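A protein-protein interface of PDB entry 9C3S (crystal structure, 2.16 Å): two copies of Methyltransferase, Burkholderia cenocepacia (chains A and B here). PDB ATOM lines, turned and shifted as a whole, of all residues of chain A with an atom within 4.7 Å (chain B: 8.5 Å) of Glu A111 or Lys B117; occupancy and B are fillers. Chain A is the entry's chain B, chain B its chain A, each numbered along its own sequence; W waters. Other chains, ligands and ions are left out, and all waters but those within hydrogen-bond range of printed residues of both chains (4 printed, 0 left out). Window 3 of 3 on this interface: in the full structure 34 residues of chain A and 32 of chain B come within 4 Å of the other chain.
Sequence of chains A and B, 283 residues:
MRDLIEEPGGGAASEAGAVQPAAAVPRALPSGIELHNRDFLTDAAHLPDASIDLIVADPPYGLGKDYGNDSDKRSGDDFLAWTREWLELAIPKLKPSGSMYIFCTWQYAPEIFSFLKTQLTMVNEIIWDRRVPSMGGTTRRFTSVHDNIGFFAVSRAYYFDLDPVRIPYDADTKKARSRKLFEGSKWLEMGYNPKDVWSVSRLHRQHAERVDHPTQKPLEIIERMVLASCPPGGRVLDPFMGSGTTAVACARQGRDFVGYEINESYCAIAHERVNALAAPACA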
ATOM      1  N   LEU A  80      18.107  38.245  16.127  1.00  0.00           N
ATOM      2  CA  LEU A  80      17.243  38.779  17.177  1.00  0.00           C
ATOM      3  C   LEU A  80      17.426  40.284  17.342  1.00  0.00           C
ATOM      4  O   LEU A  80      16.461  41.006  17.627  1.00  0.00           O
ATOM      5  CB  LEU A  80      17.509  38.057  18.494  1.00  0.00           C
ATOM      6  CG  LEU A  80      16.913  36.652  18.564  1.00  0.00           C
ATOM      7  CD1 LEU A  80      17.351  35.969  19.840  1.00  0.00           C
ATOM      8  CD2 LEU A  80      15.395  36.700  18.469  1.00  0.00           C
ATOM      9  N   GLN A 107      12.262  28.288  17.233  1.00  0.00           N
ATOM     10  CA  GLN A 107      13.686  28.450  17.500  1.00  0.00           C
ATOM     11  C   GLN A 107      13.992  29.827  18.072  1.00  0.00           C
ATOM     12  O   GLN A 107      14.931  29.975  18.861  1.00  0.00           O
ATOM     13  CB  GLN A 107      14.495  28.219  16.222  1.00  0.00           C
ATOM     14  CG  GLN A 107      14.426  26.800  15.678  1.00  0.00           C
ATOM     15  CD  GLN A 107      15.380  26.575  14.518  1.00  0.00           C
ATOM     16  OE1 GLN A 107      16.588  26.776  14.645  1.00  0.00           O
ATOM     17  NE2 GLN A 107      14.840  26.155  13.378  1.00  0.00           N
ATOM     18  N   TYR A 108      13.211  30.841  17.693  1.00  0.00           N
ATOM     19  CA  TYR A 108      13.410  32.201  18.173  1.00  0.00           C
ATOM     20  C   TYR A 108      12.184  32.775  18.868  1.00  0.00           C
ATOM     21  O   TYR A 108      12.234  33.923  19.329  1.00  0.00           O
ATOM     22  CB  TYR A 108      13.809  33.116  17.007  1.00  0.00           C
ATOM     23  CG  TYR A 108      15.093  32.692  16.332  1.00  0.00           C
ATOM     24  CD1 TYR A 108      16.318  32.902  16.945  1.00  0.00           C
ATOM     25  CD2 TYR A 108      15.077  32.074  15.090  1.00  0.00           C
ATOM     26  CE1 TYR A 108      17.495  32.514  16.338  1.00  0.00           C
ATOM     27  CE2 TYR A 108      16.251  31.683  14.475  1.00  0.00           C
ATOM     28  CZ  TYR A 108      17.456  31.904  15.104  1.00  0.00           C
ATOM     29  OH  TYR A 108      18.628  31.514  14.494  1.00  0.00           O
ATOM     30  N   ALA A 109      11.093  32.019  18.965  1.00  0.00           N
ATOM     31  CA  ALA A 109       9.882  32.554  19.577  1.00  0.00           C
ATOM     32  C   ALA A 109      10.057  32.904  21.048  1.00  0.00           C
ATOM     33  O   ALA A 109       9.573  33.972  21.459  1.00  0.00           O
ATOM     34  CB  ALA A 109       8.729  31.562  19.395  1.00  0.00           C
ATOM     35  N   PRO A 110      10.684  32.074  21.888  1.00  0.00           N
ATOM     36  CA  PRO A 110      10.856  32.475  23.297  1.00  0.00           C
ATOM     37  C   PRO A 110      11.499  33.841  23.464  1.00  0.00           C
ATOM     38  O   PRO A 110      10.964  34.684  24.193  1.00  0.00           O
ATOM     39  CB  PRO A 110      11.726  31.347  23.881  1.00  0.00           C
ATOM     40  CG  PRO A 110      11.946  30.351  22.770  1.00  0.00           C
ATOM     41  CD  PRO A 110      10.979  30.650  21.686  1.00  0.00           C
ATOM     42  N   GLU A 111      12.618  34.093  22.782  1.00  0.00           N
ATOM     43  CA  GLU A 111      13.302  35.377  22.919  1.00  0.00           C
ATOM     44  C   GLU A 111      12.435  36.520  22.405  1.00  0.00           C
ATOM     45  O   GLU A 111      12.309  37.567  23.054  1.00  0.00           O
ATOM     46  CB  GLU A 111      14.634  35.341  22.168  1.00  0.00           C
ATOM     47  CG  GLU A 111      15.655  34.366  22.739  1.00  0.00           C
ATOM     48  CD  GLU A 111      15.342  32.924  22.392  1.00  0.00           C
ATOM     49  OE1 GLU A 111      15.682  32.028  23.194  1.00  0.00           O
ATOM     50  OE2 GLU A 111      14.747  32.683  21.320  1.00  0.00           O
ATOM     51  N   ILE A 112      11.827  36.337  21.230  1.00  0.00           N
ATOM     52  CA  ILE A 112      11.048  37.412  20.620  1.00  0.00           C
ATOM     53  C   ILE A 112       9.861  37.775  21.505  1.00  0.00           C
ATOM     54  O   ILE A 112       9.606  38.953  21.789  1.00  0.00           O
ATOM     55  CB  ILE A 112      10.601  37.005  19.205  1.00  0.00           C
ATOM     56  CG1 ILE A 112      11.814  36.945  18.272  1.00  0.00           C
ATOM     57  CG2 ILE A 112       9.559  37.984  18.682  1.00  0.00           C
ATOM     58  CD1 ILE A 112      11.554  36.233  16.958  1.00  0.00           C
ATOM     59  N   PHE A 113       9.110  36.763  21.949  1.00  0.00           N
ATOM     60  CA  PHE A 113       7.952  37.022  22.797  1.00  0.00           C
ATOM     61  C   PHE A 113       8.368  37.576  24.153  1.00  0.00           C
ATOM     62  O   PHE A 113       7.665  38.427  24.714  1.00  0.00           O
ATOM     63  CB  PHE A 113       7.132  35.743  22.964  1.00  0.00           C
ATOM     64  CG  PHE A 113       6.495  35.251  21.688  1.00  0.00           C
ATOM     65  CD1 PHE A 113       6.596  35.976  20.509  1.00  0.00           C
ATOM     66  CD2 PHE A 113       5.791  34.060  21.673  1.00  0.00           C
ATOM     67  CE1 PHE A 113       6.004  35.518  19.345  1.00  0.00           C
ATOM     68  CE2 PHE A 113       5.201  33.598  20.512  1.00  0.00           C
ATOM     69  CZ  PHE A 113       5.311  34.327  19.347  1.00  0.00           C
ATOM     70  N   SER A 114       9.512  37.132  24.683  1.00  0.00           N
ATOM     71  CA  SER A 114      10.011  37.702  25.926  1.00  0.00           C
ATOM     72  C   SER A 114      10.297  39.187  25.768  1.00  0.00           C
ATOM     73  O   SER A 114       9.986  39.986  26.659  1.00  0.00           O
ATOM     74  CB  SER A 114      11.268  36.956  26.368  1.00  0.00           C
ATOM     75  OG  SER A 114      10.937  35.693  26.920  1.00  0.00           O
ATOM     76  N   PHE A 115      10.884  39.580  24.635  1.00  0.00           N
ATOM     77  CA  PHE A 115      11.168  40.997  24.434  1.00  0.00           C
ATOM     78  C   PHE A 115       9.882  41.789  24.250  1.00  0.00           C
ATOM     79  O   PHE A 115       9.749  42.900  24.777  1.00  0.00           O
ATOM     80  CB  PHE A 115      12.083  41.209  23.230  1.00  0.00           C
ATOM     81  CG  PHE A 115      12.144  42.642  22.776  1.00  0.00           C
ATOM     82  CD1 PHE A 115      12.854  43.580  23.506  1.00  0.00           C
ATOM     83  CD2 PHE A 115      11.475  43.054  21.636  1.00  0.00           C
ATOM     84  CE1 PHE A 115      12.907  44.899  23.102  1.00  0.00           C
ATOM     85  CE2 PHE A 115      11.524  44.373  21.226  1.00  0.00           C
ATOM     86  CZ  PHE A 115      12.242  45.297  21.962  1.00  0.00           C
ATOM     87  N   ILE B  91      18.102  19.688  36.563  1.00  0.00           N
ATOM     88  CA  ILE B  91      18.947  19.487  35.381  1.00  0.00           C
ATOM     89  C   ILE B  91      20.169  18.628  35.693  1.00  0.00           C
ATOM     90  O   ILE B  91      20.429  17.671  34.946  1.00  0.00           O
ATOM     91  CB  ILE B  91      19.324  20.844  34.761  1.00  0.00           C
ATOM     92  CG1 ILE B  91      18.090  21.509  34.144  1.00  0.00           C
ATOM     93  CG2 ILE B  91      20.410  20.655  33.698  1.00  0.00           C
ATOM     94  CD1 ILE B  91      18.329  22.924  33.636  1.00  0.00           C
ATOM     95  N   ALA B 109       5.643  30.333  28.850  1.00  0.00           N
ATOM     96  CA  ALA B 109       6.503  29.551  27.941  1.00  0.00           C
ATOM     97  C   ALA B 109       7.678  30.372  27.415  1.00  0.00           C
ATOM     98  O   ALA B 109       8.708  29.793  27.308  1.00  0.00           O
ATOM     99  CB  ALA B 109       5.684  28.996  26.811  1.00  0.00           C
ATOM    100  N   PRO B 110       7.565  31.623  26.938  1.00  0.00           N
ATOM    101  CA  PRO B 110       8.745  32.324  26.408  1.00  0.00           C
ATOM    102  C   PRO B 110       9.850  32.493  27.432  1.00  0.00           C
ATOM    103  O   PRO B 110      11.012  32.217  27.119  1.00  0.00           O
ATOM    104  CB  PRO B 110       8.183  33.673  25.923  1.00  0.00           C
ATOM    105  CG  PRO B 110       6.779  33.746  26.405  1.00  0.00           C
ATOM    106  CD  PRO B 110       6.316  32.355  26.676  1.00  0.00           C
ATOM    107  N   GLU B 111       9.527  32.900  28.661  1.00  0.00           N
ATOM    108  CA  GLU B 111      10.569  33.084  29.671  1.00  0.00           C
ATOM    109  C   GLU B 111      11.195  31.750  30.070  1.00  0.00           C
ATOM    110  O   GLU B 111      12.422  31.637  30.180  1.00  0.00           O
ATOM    111  CB  GLU B 111       9.993  33.791  30.898  1.00  0.00           C
ATOM    112  CG  GLU B 111       9.712  35.274  30.695  1.00  0.00           C
ATOM    113  CD  GLU B 111       8.415  35.532  29.948  1.00  0.00           C
ATOM    114  OE1 GLU B 111       7.536  34.644  29.944  1.00  0.00           O
ATOM    115  OE2 GLU B 111       8.270  36.632  29.375  1.00  0.00           O
ATOM    116  N   ILE B 112      10.367  30.730  30.307  1.00  0.00           N
ATOM    117  CA  ILE B 112      10.885  29.438  30.758  1.00  0.00           C
ATOM    118  C   ILE B 112      11.803  28.835  29.701  1.00  0.00           C
ATOM    119  O   ILE B 112      12.898  28.344  30.004  1.00  0.00           O
ATOM    120  CB  ILE B 112       9.720  28.491  31.103  1.00  0.00           C
ATOM    121  CG1 ILE B 112       9.009  28.962  32.375  1.00  0.00           C
ATOM    122  CG2 ILE B 112      10.226  27.070  31.279  1.00  0.00           C
ATOM    123  CD1 ILE B 112       7.651  28.325  32.582  1.00  0.00           C
ATOM    124  N   PHE B 113      11.369  28.860  28.442  1.00  0.00           N
ATOM    125  CA  PHE B 113      12.191  28.335  27.358  1.00  0.00           C
ATOM    126  C   PHE B 113      13.440  29.184  27.146  1.00  0.00           C
ATOM    127  O   PHE B 113      14.527  28.646  26.898  1.00  0.00           O
ATOM    128  CB  PHE B 113      11.368  28.260  26.071  1.00  0.00           C
ATOM    129  CG  PHE B 113      10.234  27.263  26.119  1.00  0.00           C
ATOM    130  CD1 PHE B 113      10.072  26.409  27.201  1.00  0.00           C
ATOM    131  CD2 PHE B 113       9.331  27.181  25.074  1.00  0.00           C
ATOM    132  CE1 PHE B 113       9.034  25.499  27.236  1.00  0.00           C
ATOM    133  CE2 PHE B 113       8.290  26.273  25.106  1.00  0.00           C
ATOM    134  CZ  PHE B 113       8.143  25.431  26.188  1.00  0.00           C
ATOM    135  N   SER B 114      13.309  30.512  27.227  1.00  0.00           N
ATOM    136  CA  SER B 114      14.476  31.377  27.114  1.00  0.00           C
ATOM    137  C   SER B 114      15.512  31.026  28.169  1.00  0.00           C
ATOM    138  O   SER B 114      16.716  31.017  27.891  1.00  0.00           O
ATOM    139  CB  SER B 114      14.048  32.840  27.249  1.00  0.00           C
ATOM    140  OG  SER B 114      13.418  33.298  26.064  1.00  0.00           O
ATOM    141  N   PHE B 115      15.058  30.727  29.387  1.00  0.00           N
ATOM    142  CA  PHE B 115      15.993  30.375  30.449  1.00  0.00           C
ATOM    143  C   PHE B 115      16.595  28.996  30.218  1.00  0.00           C
ATOM    144  O   PHE B 115      17.788  28.785  30.464  1.00  0.00           O
ATOM    145  CB  PHE B 115      15.294  30.415  31.806  1.00  0.00           C
ATOM    146  CG  PHE B 115      16.001  29.619  32.860  1.00  0.00           C
ATOM    147  CD1 PHE B 115      17.136  30.118  33.470  1.00  0.00           C
ATOM    148  CD2 PHE B 115      15.544  28.364  33.226  1.00  0.00           C
ATOM    149  CE1 PHE B 115      17.799  29.388  34.436  1.00  0.00           C
ATOM    150  CE2 PHE B 115      16.202  27.628  34.191  1.00  0.00           C
ATOM    151  CZ  PHE B 115      17.332  28.141  34.796  1.00  0.00           C
ATOM    152  N   LEU B 116      15.788  28.045  29.752  1.00  0.00           N
ATOM    153  CA  LEU B 116      16.292  26.692  29.553  1.00  0.00           C
ATOM    154  C   LEU B 116      17.286  26.622  28.407  1.00  0.00           C
ATOM    155  O   LEU B 116      18.161  25.749  28.400  1.00  0.00           O
ATOM    156  CB  LEU B 116      15.131  25.734  29.302  1.00  0.00           C
ATOM    157  CG  LEU B 116      14.361  25.379  30.570  1.00  0.00           C
ATOM    158  CD1 LEU B 116      13.193  24.468  30.271  1.00  0.00           C
ATOM    159  CD2 LEU B 116      15.310  24.716  31.534  1.00  0.00           C
ATOM    160  N   LYS B 117      17.167  27.518  27.430  1.00  0.00           N
ATOM    161  CA  LYS B 117      18.111  27.511  26.322  1.00  0.00           C
ATOM    162  C   LYS B 117      19.521  27.865  26.771  1.00  0.00           C
ATOM    163  O   LYS B 117      20.486  27.466  26.111  1.00  0.00           O
ATOM    164  CB  LYS B 117      17.638  28.471  25.232  1.00  0.00           C
ATOM    165  CG  LYS B 117      16.622  27.842  24.293  1.00  0.00           C
ATOM    166  CD  LYS B 117      15.852  28.877  23.495  1.00  0.00           C
ATOM    167  CE  LYS B 117      16.525  29.165  22.169  1.00  0.00           C
ATOM    168  NZ  LYS B 117      15.766  30.174  21.392  1.00  0.00           N
ATOM    169  N   THR B 118      19.662  28.595  27.882  1.00  0.00           N
ATOM    170  CA  THR B 118      20.977  28.897  28.432  1.00  0.00           C
ATOM    171  C   THR B 118      21.584  27.714  29.173  1.00  0.00           C
ATOM    172  O   THR B 118      22.800  27.690  29.388  1.00  0.00           O
ATOM    173  CB  THR B 118      20.899  30.094  29.384  1.00  0.00           C
ATOM    174  OG1 THR B 118      20.221  29.711  30.589  1.00  0.00           O
ATOM    175  CG2 THR B 118      20.170  31.266  28.734  1.00  0.00           C
ATOM    176  N   GLN B 119      20.766  26.743  29.573  1.00  0.00           N
ATOM    177  CA  GLN B 119      21.232  25.561  30.282  1.00  0.00           C
ATOM    178  C   GLN B 119      21.268  24.322  29.408  1.00  0.00           C
ATOM    179  O   GLN B 119      22.116  23.453  29.620  1.00  0.00           O
ATOM    180  CB  GLN B 119      20.329  25.275  31.489  1.00  0.00           C
ATOM    181  CG  GLN B 119      20.146  26.459  32.425  1.00  0.00           C
ATOM    182  CD  GLN B 119      21.225  26.537  33.485  1.00  0.00           C
ATOM    183  OE1 GLN B 119      21.706  25.516  33.978  1.00  0.00           O
ATOM    184  NE2 GLN B 119      21.612  27.756  33.841  1.00  0.00           N
ATOM    185  N   LEU B 120      20.363  24.226  28.438  1.00  0.00           N
ATOM    186  CA  LEU B 120      20.266  23.077  27.555  1.00  0.00           C
ATOM    187  C   LEU B 120      20.007  23.576  26.143  1.00  0.00           C
ATOM    188  O   LEU B 120      19.814  24.773  25.908  1.00  0.00           O
ATOM    189  CB  LEU B 120      19.151  22.123  27.997  1.00  0.00           C
ATOM    190  CG  LEU B 120      19.147  21.714  29.470  1.00  0.00           C
ATOM    191  CD1 LEU B 120      17.724  21.633  29.994  1.00  0.00           C
ATOM    192  CD2 LEU B 120      19.867  20.392  29.646  1.00  0.00           C
ATOM    193  N   THR B 121      19.998  22.641  25.198  1.00  0.00           N
ATOM    194  CA  THR B 121      19.687  22.929  23.806  1.00  0.00           C
ATOM    195  C   THR B 121      18.290  22.412  23.495  1.00  0.00           C
ATOM    196  O   THR B 121      17.957  21.272  23.836  1.00  0.00           O
ATOM    197  CB  THR B 121      20.713  22.287  22.867  1.00  0.00           C
ATOM    198  OG1 THR B 121      20.374  20.913  22.649  1.00  0.00           O
ATOM    199  CG2 THR B 121      22.117  22.374  23.462  1.00  0.00           C
ATOM    200  N   MET B 122      17.478  23.252  22.853  1.00  0.00           N
ATOM    201  CA  MET B 122      16.103  22.888  22.539  1.00  0.00           C
ATOM    202  C   MET B 122      16.065  22.012  21.298  1.00  0.00           C
ATOM    203  O   MET B 122      16.537  22.415  20.229  1.00  0.00           O
ATOM    204  CB  MET B 122      15.245  24.130  22.319  1.00  0.00           C
ATOM    205  CG  MET B 122      13.792  23.932  22.732  1.00  0.00           C
ATOM    206  SD  MET B 122      12.955  25.477  23.124  1.00  0.00           S
ATOM    207  CE  MET B 122      11.256  25.057  22.778  1.00  0.00           C
ATOM    208  N   VAL B 123      15.486  20.823  21.436  1.00  0.00           N
ATOM    209  CA  VAL B 123      15.302  19.943  20.291  1.00  0.00           C
ATOM    210  C   VAL B 123      13.934  20.143  19.648  1.00  0.00           C
ATOM    211  O   VAL B 123      13.788  19.948  18.436  1.00  0.00           O
ATOM    212  CB  VAL B 123      15.490  18.478  20.706  1.00  0.00           C
ATOM    213  CG1 VAL B 123      15.252  17.566  19.518  1.00  0.00           C
ATOM    214  CG2 VAL B 123      16.875  18.265  21.279  1.00  0.00           C
ATOM    215  N   PHE B 151      11.078  20.526  24.575  1.00  0.00           N
ATOM    216  CA  PHE B 151      11.877  19.310  24.472  1.00  0.00           C
ATOM    217  C   PHE B 151      13.334  19.732  24.337  1.00  0.00           C
ATOM    218  O   PHE B 151      13.742  20.221  23.275  1.00  0.00           O
ATOM    219  CB  PHE B 151      11.423  18.483  23.270  1.00  0.00           C
ATOM    220  CG  PHE B 151      12.212  17.220  23.054  1.00  0.00           C
ATOM    221  CD1 PHE B 151      12.733  16.513  24.123  1.00  0.00           C
ATOM    222  CD2 PHE B 151      12.423  16.734  21.771  1.00  0.00           C
ATOM    223  CE1 PHE B 151      13.454  15.350  23.918  1.00  0.00           C
ATOM    224  CE2 PHE B 151      13.143  15.574  21.561  1.00  0.00           C
ATOM    225  CZ  PHE B 151      13.658  14.881  22.636  1.00  0.00           C
ATOM    226  N   PHE B 152      14.103  19.538  25.412  1.00  0.00           N
ATOM    227  CA  PHE B 152      15.495  19.955  25.509  1.00  0.00           C
ATOM    228  C   PHE B 152      16.405  18.746  25.682  1.00  0.00           C
ATOM    229  O   PHE B 152      15.974  17.669  26.109  1.00  0.00           O
ATOM    230  CB  PHE B 152      15.721  20.899  26.695  1.00  0.00           C
ATOM    231  CG  PHE B 152      14.878  22.133  26.662  1.00  0.00           C
ATOM    232  CD1 PHE B 152      13.605  22.131  27.204  1.00  0.00           C
ATOM    233  CD2 PHE B 152      15.364  23.301  26.104  1.00  0.00           C
ATOM    234  CE1 PHE B 152      12.827  23.269  27.181  1.00  0.00           C
ATOM    235  CE2 PHE B 152      14.593  24.443  26.076  1.00  0.00           C
ATOM    236  CZ  PHE B 152      13.322  24.427  26.616  1.00  0.00           C
ATOM    237  N   ALA B 153      17.686  18.954  25.384  1.00  0.00           N
ATOM    238  CA  ALA B 153      18.696  17.912  25.486  1.00  0.00           C
ATOM    239  C   ALA B 153      19.968  18.496  26.079  1.00  0.00           C
ATOM    240  O   ALA B 153      20.316  19.648  25.803  1.00  0.00           O
ATOM    241  CB  ALA B 153      18.993  17.293  24.116  1.00  0.00           C
ATOM    242  N   ARG B 156      24.410  17.100  22.227  1.00  0.00           N
ATOM    243  CA  ARG B 156      23.919  16.921  20.872  1.00  0.00           C
ATOM    244  C   ARG B 156      23.828  15.447  20.498  1.00  0.00           C
ATOM    245  O   ARG B 156      23.405  15.126  19.383  1.00  0.00           O
ATOM    246  CB  ARG B 156      24.818  17.665  19.872  1.00  0.00           C
ATOM    247  CG  ARG B 156      25.540  18.971  20.354  1.00  0.00           C
ATOM    248  CD  ARG B 156      24.835  19.822  21.442  1.00  0.00           C
ATOM    249  NE  ARG B 156      25.687  20.911  21.920  1.00  0.00           N
ATOM    250  CZ  ARG B 156      25.827  21.273  23.191  1.00  0.00           C
ATOM    251  NH1 ARG B 156      25.181  20.655  24.168  1.00  0.00           N
ATOM    252  NH2 ARG B 156      26.639  22.282  23.495  1.00  0.00           N
HETATM  253  O   HOH W   1      13.350  35.842  28.297  1.00  0.00           O
HETATM  254  O   HOH W   2      14.123  27.763  20.845  1.00  0.00           O
HETATM  255  O   HOH W   3      18.372  32.111  25.427  1.00  0.00           O
HETATM  256  O   HOH W   4       9.631  39.274  29.355  1.00  0.00           O
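Among the printed residues, pairs that only touch across the chains: Pro A110 with Pro B110, Pro A110 with Phe B113, Phe A113 with Pro B110, Ser A114 with Glu B111 and Ser A114 with Ser B114.
Water W1 bridges the side-chain hydroxyl (OG) of Ser A114 (2.8 Å) and the side-chain hydroxyl (OG) of Ser B114 (3.4 Å). Water W4 lies within hydrogen-bond range of O of Ser A114 (2.8 Å) and OE2 of Glu B111 (3.0 Å). Water W2 lies within hydrogen-bond range of NZ of Lys B117 (3.0 Å), O of Gln A107 (3.1 Å) and SD of Met B122 (3.4 Å). Water W3 bridges O of Ser B114 and OE1 of Glu A111.
Pro B110 touches its own counterpart, Pro A110. Pro A110 touches Phe B113, and with the chains exchanged Phe A113 touches Pro B110. Pro A110 touches Ser B114, and with the chains exchanged Ser A114 touches Pro B110. Ser A114 touches its own counterpart, Ser B114. Positions printed for both chains: 109, 110, 111, 112, 113, 114 and 115.
Hydrophobic or aromatic side chains of chain A within 4 Å of the printed part of chain B: Pro A110 and Phe A113. Of the 20 printed residues of chain B, 5 touch a printed residue of chain A. Hydrophobic or aromatic side chains of chain B that line the printed part of chain A: Pro B110 and Phe B113. Among the printed residues, Asp or Glu carboxylates within 4 Å of a Lys or Arg side-chain nitrogen of the other chain: Glu A111 with Lys B117 (2.6 Å).
Of chain B, only Ser B114 (3.5 Å) and Lys B117 (2.6 Å) come within 4 Å of Glu A111. Of chain A, only Gln A107 (2.7 Å) and Glu A111 (2.6 Å) come within 4 Å of Lys B117. Printed residues of chain A within 4 Å of Ser B114: Pro A110, Glu A111 and Ser A114. Of the printed residues of chain A, Phe B113 touches Pro A110. Of the printed residues of chain A, Pro B110 touches Pro A110 (3.4 Å), Phe A113 (3.8 Å) and Ser A114 (3.4 Å). The nearest residue of chain A that does not touch Lys B117 is Pro A110 (4.1 Å). The nearest printed residue of chain A that does not touch Pro B110 is Ala A109 (4.7 Å).
The side-chain hydroxyl of Ser B114 sits close to the backbone carbonyl oxygen of Pro A110 (3.4 Å). NZ of Lys B117 is in hydrogen-bond range of O of Gln A107 (2.7 Å). The backbone NH (N) of Glu A111 sits at hydrogen-bond distance from the side-chain hydroxyl (OG) of Ser B114 (3.5 Å). OG of Ser A114 sits close to O of Pro B110 (3.5 Å). NZ of Lys B117 lies within salt-bridge range of OE1 of Glu A111.
O of Pro B110 lies within hydrogen-bond range of OG of Ser B114 (2.8 Å). The backbone carbonyl oxygen (O) of Pro A110 lies within hydrogen-bond range of the side-chain hydroxyl (OG) of Ser A114 (2.9 Å).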
